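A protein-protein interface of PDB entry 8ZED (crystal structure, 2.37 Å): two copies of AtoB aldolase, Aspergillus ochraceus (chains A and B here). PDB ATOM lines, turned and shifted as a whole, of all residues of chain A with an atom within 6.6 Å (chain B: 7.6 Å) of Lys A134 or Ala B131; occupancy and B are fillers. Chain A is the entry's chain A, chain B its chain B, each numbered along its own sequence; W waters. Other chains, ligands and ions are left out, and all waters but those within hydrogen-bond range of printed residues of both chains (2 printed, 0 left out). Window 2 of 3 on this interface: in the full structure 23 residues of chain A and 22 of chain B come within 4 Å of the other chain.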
ATOM      1  N   SER A  43      24.781  -9.645 -18.148  1.00  0.00           N
ATOM      2  CA  SER A  43      26.146  -9.141 -18.054  1.00  0.00           C
ATOM      3  C   SER A  43      27.046 -10.056 -17.234  1.00  0.00           C
ATOM      4  O   SER A  43      28.272  -9.980 -17.368  1.00  0.00           O
ATOM      5  CB  SER A  43      26.151  -7.736 -17.451  1.00  0.00           C
ATOM      6  OG  SER A  43      25.661  -7.753 -16.121  1.00  0.00           O
ATOM      7  N   PHE A  44      26.467 -10.912 -16.389  1.00  0.00           N
ATOM      8  CA  PHE A  44      27.280 -11.821 -15.590  1.00  0.00           C
ATOM      9  C   PHE A  44      27.972 -12.866 -16.459  1.00  0.00           C
ATOM     10  O   PHE A  44      29.057 -13.343 -16.106  1.00  0.00           O
ATOM     11  CB  PHE A  44      26.417 -12.490 -14.520  1.00  0.00           C
ATOM     12  CG  PHE A  44      27.200 -13.289 -13.522  1.00  0.00           C
ATOM     13  CD1 PHE A  44      28.061 -12.662 -12.638  1.00  0.00           C
ATOM     14  CD2 PHE A  44      27.069 -14.665 -13.461  1.00  0.00           C
ATOM     15  CE1 PHE A  44      28.783 -13.393 -11.716  1.00  0.00           C
ATOM     16  CE2 PHE A  44      27.787 -15.403 -12.539  1.00  0.00           C
ATOM     17  CZ  PHE A  44      28.646 -14.766 -11.666  1.00  0.00           C
ATOM     18  N   ASP A 129      23.615 -11.337  -7.283  1.00  0.00           N
ATOM     19  CA  ASP A 129      24.488 -10.253  -6.834  1.00  0.00           C
ATOM     20  C   ASP A 129      25.810 -10.366  -7.584  1.00  0.00           C
ATOM     21  O   ASP A 129      26.688 -11.143  -7.206  1.00  0.00           O
ATOM     22  CB  ASP A 129      24.694 -10.337  -5.325  1.00  0.00           C
ATOM     23  CG  ASP A 129      25.359  -9.100  -4.747  1.00  0.00           C
ATOM     24  OD1 ASP A 129      26.044  -8.369  -5.492  1.00  0.00           O
ATOM     25  OD2 ASP A 129      25.201  -8.860  -3.531  1.00  0.00           O
ATOM     26  N   THR A 130      25.960  -9.574  -8.648  1.00  0.00           N
ATOM     27  CA  THR A 130      27.101  -9.739  -9.544  1.00  0.00           C
ATOM     28  C   THR A 130      28.418  -9.392  -8.860  1.00  0.00           C
ATOM     29  O   THR A 130      29.437 -10.048  -9.104  1.00  0.00           O
ATOM     30  CB  THR A 130      26.913  -8.885 -10.796  1.00  0.00           C
ATOM     31  OG1 THR A 130      26.532  -7.556 -10.418  1.00  0.00           O
ATOM     32  CG2 THR A 130      25.840  -9.482 -11.691  1.00  0.00           C
ATOM     33  N   ALA A 131      28.424  -8.363  -8.008  1.00  0.00           N
ATOM     34  CA  ALA A 131      29.673  -7.932  -7.387  1.00  0.00           C
ATOM     35  C   ALA A 131      30.240  -9.008  -6.470  1.00  0.00           C
ATOM     36  O   ALA A 131      31.458  -9.212  -6.418  1.00  0.00           O
ATOM     37  CB  ALA A 131      29.459  -6.630  -6.617  1.00  0.00           C
ATOM     38  N   ALA A 132      29.372  -9.710  -5.738  1.00  0.00           N
ATOM     39  CA  ALA A 132      29.843 -10.741  -4.821  1.00  0.00           C
ATOM     40  C   ALA A 132      30.197 -12.029  -5.553  1.00  0.00           C
ATOM     41  O   ALA A 132      31.157 -12.713  -5.181  1.00  0.00           O
ATOM     42  CB  ALA A 132      28.790 -11.008  -3.745  1.00  0.00           C
ATOM     43  N   GLU A 133      29.435 -12.377  -6.594  1.00  0.00           N
ATOM     44  CA  GLU A 133      29.702 -13.617  -7.318  1.00  0.00           C
ATOM     45  C   GLU A 133      30.970 -13.508  -8.157  1.00  0.00           C
ATOM     46  O   GLU A 133      31.716 -14.485  -8.290  1.00  0.00           O
ATOM     47  CB  GLU A 133      28.505 -13.981  -8.195  1.00  0.00           C
ATOM     48  CG  GLU A 133      27.217 -14.226  -7.424  1.00  0.00           C
ATOM     49  CD  GLU A 133      27.204 -15.550  -6.687  1.00  0.00           C
ATOM     50  OE1 GLU A 133      28.098 -16.386  -6.938  1.00  0.00           O
ATOM     51  OE2 GLU A 133      26.293 -15.755  -5.859  1.00  0.00           O
ATOM     52  N   LYS A 134      31.227 -12.334  -8.740  1.00  0.00           N
ATOM     53  CA  LYS A 134      32.491 -12.127  -9.440  1.00  0.00           C
ATOM     54  C   LYS A 134      33.666 -12.211  -8.475  1.00  0.00           C
ATOM     55  O   LYS A 134      34.736 -12.721  -8.827  1.00  0.00           O
ATOM     56  CB  LYS A 134      32.487 -10.775 -10.156  1.00  0.00           C
ATOM     57  CG  LYS A 134      31.565 -10.696 -11.360  1.00  0.00           C
ATOM     58  CD  LYS A 134      31.607  -9.306 -11.978  1.00  0.00           C
ATOM     59  CE  LYS A 134      30.654  -9.184 -13.156  1.00  0.00           C
ATOM     60  NZ  LYS A 134      30.682  -7.814 -13.741  1.00  0.00           N
ATOM     61  N   LYS A 135      33.480 -11.716  -7.250  1.00  0.00           N
ATOM     62  CA  LYS A 135      34.541 -11.780  -6.250  1.00  0.00           C
ATOM     63  C   LYS A 135      34.765 -13.212  -5.779  1.00  0.00           C
ATOM     64  O   LYS A 135      35.901 -13.608  -5.498  1.00  0.00           O
ATOM     65  CB  LYS A 135      34.196 -10.864  -5.075  1.00  0.00           C
ATOM     66  CG  LYS A 135      35.301 -10.693  -4.045  1.00  0.00           C
ATOM     67  CD  LYS A 135      35.049 -11.539  -2.808  1.00  0.00           C
ATOM     68  CE  LYS A 135      35.344 -10.754  -1.540  1.00  0.00           C
ATOM     69  NZ  LYS A 135      36.723 -10.194  -1.538  1.00  0.00           N
ATOM     70  N   PHE A 136      33.692 -14.001  -5.690  1.00  0.00           N
ATOM     71  CA  PHE A 136      33.833 -15.400  -5.300  1.00  0.00           C
ATOM     72  C   PHE A 136      34.533 -16.205  -6.387  1.00  0.00           C
ATOM     73  O   PHE A 136      35.380 -17.056  -6.091  1.00  0.00           O
ATOM     74  CB  PHE A 136      32.460 -15.995  -4.989  1.00  0.00           C
ATOM     75  CG  PHE A 136      32.509 -17.409  -4.479  1.00  0.00           C
ATOM     76  CD1 PHE A 136      33.564 -17.843  -3.693  1.00  0.00           C
ATOM     77  CD2 PHE A 136      31.500 -18.305  -4.792  1.00  0.00           C
ATOM     78  CE1 PHE A 136      33.610 -19.144  -3.227  1.00  0.00           C
ATOM     79  CE2 PHE A 136      31.542 -19.607  -4.329  1.00  0.00           C
ATOM     80  CZ  PHE A 136      32.598 -20.026  -3.545  1.00  0.00           C
ATOM     81  N   ALA A 137      34.197 -15.946  -7.653  1.00  0.00           N
ATOM     82  CA  ALA A 137      34.808 -16.691  -8.750  1.00  0.00           C
ATOM     83  C   ALA A 137      36.288 -16.361  -8.888  1.00  0.00           C
ATOM     84  O   ALA A 137      37.110 -17.256  -9.122  1.00  0.00           O
ATOM     85  CB  ALA A 137      34.068 -16.402 -10.055  1.00  0.00           C
ATOM     86  N   ALA A 138      36.648 -15.090  -8.747  1.00  0.00           N
ATOM     87  CA  ALA A 138      38.041 -14.673  -8.864  1.00  0.00           C
ATOM     88  C   ALA A 138      38.791 -14.908  -7.557  1.00  0.00           C
ATOM     89  O   ALA A 138      38.786 -16.015  -7.017  1.00  0.00           O
ATOM     90  CB  ALA A 138      38.124 -13.211  -9.269  1.00  0.00           C
ATOM     91  N   PHE B  44      24.340  -3.727  -1.386  1.00  0.00           N
ATOM     92  CA  PHE B  44      24.753  -2.547  -2.137  1.00  0.00           C
ATOM     93  C   PHE B  44      24.876  -1.323  -1.239  1.00  0.00           C
ATOM     94  O   PHE B  44      25.673  -0.423  -1.528  1.00  0.00           O
ATOM     95  CB  PHE B  44      23.768  -2.284  -3.275  1.00  0.00           C
ATOM     96  CG  PHE B  44      24.199  -1.191  -4.208  1.00  0.00           C
ATOM     97  CD1 PHE B  44      25.300  -1.361  -5.031  1.00  0.00           C
ATOM     98  CD2 PHE B  44      23.499   0.002  -4.270  1.00  0.00           C
ATOM     99  CE1 PHE B  44      25.700  -0.358  -5.891  1.00  0.00           C
ATOM    100  CE2 PHE B  44      23.893   1.008  -5.130  1.00  0.00           C
ATOM    101  CZ  PHE B  44      24.995   0.828  -5.942  1.00  0.00           C
ATOM    102  N   ASN B 106      21.785  -0.854 -18.043  1.00  0.00           N
ATOM    103  CA  ASN B 106      21.870  -2.076 -17.253  1.00  0.00           C
ATOM    104  C   ASN B 106      20.509  -2.757 -17.238  1.00  0.00           C
ATOM    105  O   ASN B 106      19.504  -2.204 -17.690  1.00  0.00           O
ATOM    106  CB  ASN B 106      22.358  -1.796 -15.828  1.00  0.00           C
ATOM    107  CG  ASN B 106      23.835  -1.457 -15.775  1.00  0.00           C
ATOM    108  OD1 ASN B 106      24.688  -2.312 -16.014  1.00  0.00           O
ATOM    109  ND2 ASN B 106      24.145  -0.205 -15.458  1.00  0.00           N
ATOM    110  N   VAL B 128      19.481  -4.507  -8.671  1.00  0.00           N
ATOM    111  CA  VAL B 128      20.377  -3.887  -9.640  1.00  0.00           C
ATOM    112  C   VAL B 128      21.626  -4.743  -9.825  1.00  0.00           C
ATOM    113  O   VAL B 128      21.932  -5.633  -9.028  1.00  0.00           O
ATOM    114  CB  VAL B 128      20.767  -2.454  -9.222  1.00  0.00           C
ATOM    115  CG1 VAL B 128      19.526  -1.640  -8.901  1.00  0.00           C
ATOM    116  CG2 VAL B 128      21.721  -2.486  -8.032  1.00  0.00           C
ATOM    117  N   ASP B 129      22.353  -4.452 -10.905  1.00  0.00           N
ATOM    118  CA  ASP B 129      23.645  -5.074 -11.192  1.00  0.00           C
ATOM    119  C   ASP B 129      24.685  -4.433 -10.282  1.00  0.00           C
ATOM    120  O   ASP B 129      25.173  -3.336 -10.555  1.00  0.00           O
ATOM    121  CB  ASP B 129      24.003  -4.900 -12.666  1.00  0.00           C
ATOM    122  CG  ASP B 129      25.212  -5.727 -13.090  1.00  0.00           C
ATOM    123  OD1 ASP B 129      26.064  -6.052 -12.240  1.00  0.00           O
ATOM    124  OD2 ASP B 129      25.308  -6.047 -14.295  1.00  0.00           O
ATOM    125  N   THR B 130      25.038  -5.128  -9.198  1.00  0.00           N
ATOM    126  CA  THR B 130      25.919  -4.540  -8.193  1.00  0.00           C
ATOM    127  C   THR B 130      27.318  -4.290  -8.747  1.00  0.00           C
ATOM    128  O   THR B 130      27.947  -3.277  -8.419  1.00  0.00           O
ATOM    129  CB  THR B 130      25.980  -5.437  -6.958  1.00  0.00           C
ATOM    130  OG1 THR B 130      26.316  -6.774  -7.351  1.00  0.00           O
ATOM    131  CG2 THR B 130      24.640  -5.450  -6.250  1.00  0.00           C
ATOM    132  N   ALA B 131      27.821  -5.197  -9.586  1.00  0.00           N
ATOM    133  CA  ALA B 131      29.161  -5.023 -10.137  1.00  0.00           C
ATOM    134  C   ALA B 131      29.240  -3.813 -11.060  1.00  0.00           C
ATOM    135  O   ALA B 131      30.289  -3.165 -11.141  1.00  0.00           O
ATOM    136  CB  ALA B 131      29.593  -6.288 -10.879  1.00  0.00           C
ATOM    137  N   ALA B 132      28.151  -3.491 -11.757  1.00  0.00           N
ATOM    138  CA  ALA B 132      28.152  -2.356 -12.671  1.00  0.00           C
ATOM    139  C   ALA B 132      27.822  -1.040 -11.980  1.00  0.00           C
ATOM    140  O   ALA B 132      28.351   0.005 -12.375  1.00  0.00           O
ATOM    141  CB  ALA B 132      27.162  -2.596 -13.814  1.00  0.00           C
ATOM    142  N   GLU B 133      26.964  -1.065 -10.958  1.00  0.00           N
ATOM    143  CA  GLU B 133      26.618   0.169 -10.259  1.00  0.00           C
ATOM    144  C   GLU B 133      27.781   0.669  -9.412  1.00  0.00           C
ATOM    145  O   GLU B 133      28.029   1.878  -9.340  1.00  0.00           O
ATOM    146  CB  GLU B 133      25.374  -0.043  -9.396  1.00  0.00           C
ATOM    147  CG  GLU B 133      24.107  -0.358 -10.180  1.00  0.00           C
ATOM    148  CD  GLU B 133      23.550   0.845 -10.921  1.00  0.00           C
ATOM    149  OE1 GLU B 133      24.057   1.968 -10.717  1.00  0.00           O
ATOM    150  OE2 GLU B 133      22.596   0.668 -11.707  1.00  0.00           O
ATOM    151  N   LYS B 134      28.505  -0.244  -8.759  1.00  0.00           N
ATOM    152  CA  LYS B 134      29.689   0.162  -8.008  1.00  0.00           C
ATOM    153  C   LYS B 134      30.796   0.640  -8.936  1.00  0.00           C
ATOM    154  O   LYS B 134      31.649   1.435  -8.525  1.00  0.00           O
ATOM    155  CB  LYS B 134      30.173  -0.994  -7.133  1.00  0.00           C
ATOM    156  CG  LYS B 134      29.136  -1.455  -6.119  1.00  0.00           C
ATOM    157  CD  LYS B 134      29.527  -2.764  -5.456  1.00  0.00           C
ATOM    158  CE  LYS B 134      30.638  -2.567  -4.441  1.00  0.00           C
ATOM    159  NZ  LYS B 134      30.908  -3.823  -3.689  1.00  0.00           N
ATOM    160  N   LYS B 135      30.799   0.171 -10.186  1.00  0.00           N
ATOM    161  CA  LYS B 135      31.744   0.686 -11.169  1.00  0.00           C
ATOM    162  C   LYS B 135      31.343   2.074 -11.651  1.00  0.00           C
ATOM    163  O   LYS B 135      32.210   2.906 -11.939  1.00  0.00           O
ATOM    164  CB  LYS B 135      31.841  -0.278 -12.350  1.00  0.00           C
ATOM    165  CG  LYS B 135      33.060  -0.077 -13.233  1.00  0.00           C
ATOM    166  CD  LYS B 135      34.325  -0.528 -12.523  1.00  0.00           C
ATOM    167  CE  LYS B 135      35.190  -1.378 -13.438  1.00  0.00           C
ATOM    168  NZ  LYS B 135      34.483  -2.615 -13.872  1.00  0.00           N
ATOM    169  N   PHE B 136      30.037   2.338 -11.740  1.00  0.00           N
ATOM    170  CA  PHE B 136      29.569   3.640 -12.201  1.00  0.00           C
ATOM    171  C   PHE B 136      29.787   4.713 -11.142  1.00  0.00           C
ATOM    172  O   PHE B 136      30.140   5.852 -11.469  1.00  0.00           O
ATOM    173  CB  PHE B 136      28.093   3.552 -12.591  1.00  0.00           C
ATOM    174  CG  PHE B 136      27.478   4.872 -12.958  1.00  0.00           C
ATOM    175  CD1 PHE B 136      28.027   5.655 -13.960  1.00  0.00           C
ATOM    176  CD2 PHE B 136      26.337   5.324 -12.311  1.00  0.00           C
ATOM    177  CE1 PHE B 136      27.459   6.869 -14.302  1.00  0.00           C
ATOM    178  CE2 PHE B 136      25.764   6.536 -12.650  1.00  0.00           C
ATOM    179  CZ  PHE B 136      26.326   7.310 -13.646  1.00  0.00           C
HETATM  180  O   HOH W   1      28.146  -6.399 -14.260  1.00  0.00           O
HETATM  181  O   HOH W   2      23.414  -7.864  -9.130  1.00  0.00           O
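OG1 of Thr A130 sits at hydrogen-bond distance from N of Thr B130 (3.1 Å). The side-chain hydroxyl (OG1) of Thr A130 lies within hydrogen-bond range of the backbone NH (N) of Ala B131 (2.8 Å). The side-chain hydroxyl (OG1) of Thr B130 sits at hydrogen-bond distance from the backbone NH (N) of Ala A131, 2.7 Å away. The side-chain hydroxyl of Ser A43 is in hydrogen-bond range of the side-chain carboxylate of Asp B129, at 2.5 Å. The side-chain carboxylate of Asp A129 sits at hydrogen-bond distance from the side-chain hydroxyl of Thr B130, at 2.5 Å. The side-chain hydroxyl (OG1) of Thr A130 is in hydrogen-bond range of the side-chain carboxylate (OD1) of Asp B129 (2.4 Å).
OD1 of Asp B129 lies within hydrogen-bond range of N of Ala B131, at 3.3 Å. OD1 of Asp A129 lies close to N of Ala A131 (3.5 Å). OD1 of Asp B129 is in hydrogen-bond range of N of Ala B132, at 3.3 Å.
Ala A131 touches Ala B131 (N to N, 3.6 Å). NZ of Lys A134 touches CB of Ala B131 (3.4 Å).
Lys A134 touches one residue of chain B. Of chain A, only Thr A130 (2.8 Å), Ala A131 (3.6 Å) and Lys A134 (3.4 Å) come within 4 Å of Ala B131. Printed residues of chain B within 4 Å of Ser A43: Asp B129. Printed residues of chain B within 4 Å of Ala A131: Thr B130 (2.7 Å) and Ala B131 (3.6 Å). Of the printed residues of chain A, Thr B130 touches Asp A129 (2.5 Å), Thr A130 (3.1 Å) and Ala A131 (2.7 Å). Phe A136 touches none of the printed residues of chain B. The nearest printed residue of chain B that does not touch Ala A131 is Lys B134 (4.04 Å).
Hydrophobic or aromatic side chains of chain A that line the printed part of chain B: Ala A131. Among the printed residues, 8 pairs touch across the chains. Among the printed residues, no Asp or Glu carboxylate lies within 4 Å of a Lys or Arg side-chain nitrogen of the other chain.
Asp A129 touches Thr B130, and with the chains exchanged Thr A130 touches Asp B129. Thr A130 touches its own counterpart, Thr B130. Thr A130 touches Ala B131, and with the chains exchanged Ala A131 touches Thr B130. Lys A134 touches Ala B131, but with the chains exchanged Ala A131 does not touch Lys B134 (4.04 Å). Positions printed for both chains: 44, 129, 130, 131, 132, 133, 134, 135 and 136. Of the 8 pairs that touch across the chains among the printed residues, 6 have their exchanged pair printed and touching as well.
Water W2 lies within hydrogen-bond range of O of Val B128 (2.7 Å), N of Thr A130 (3.1 Å) and N of Thr B130 (3.2 Å). Water W1 lies within hydrogen-bond range of OD2 of Asp B129 (2.9 Å), NZ of Lys A134 (3.0 Å) and OG of Ser A43 (3.4 Å).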
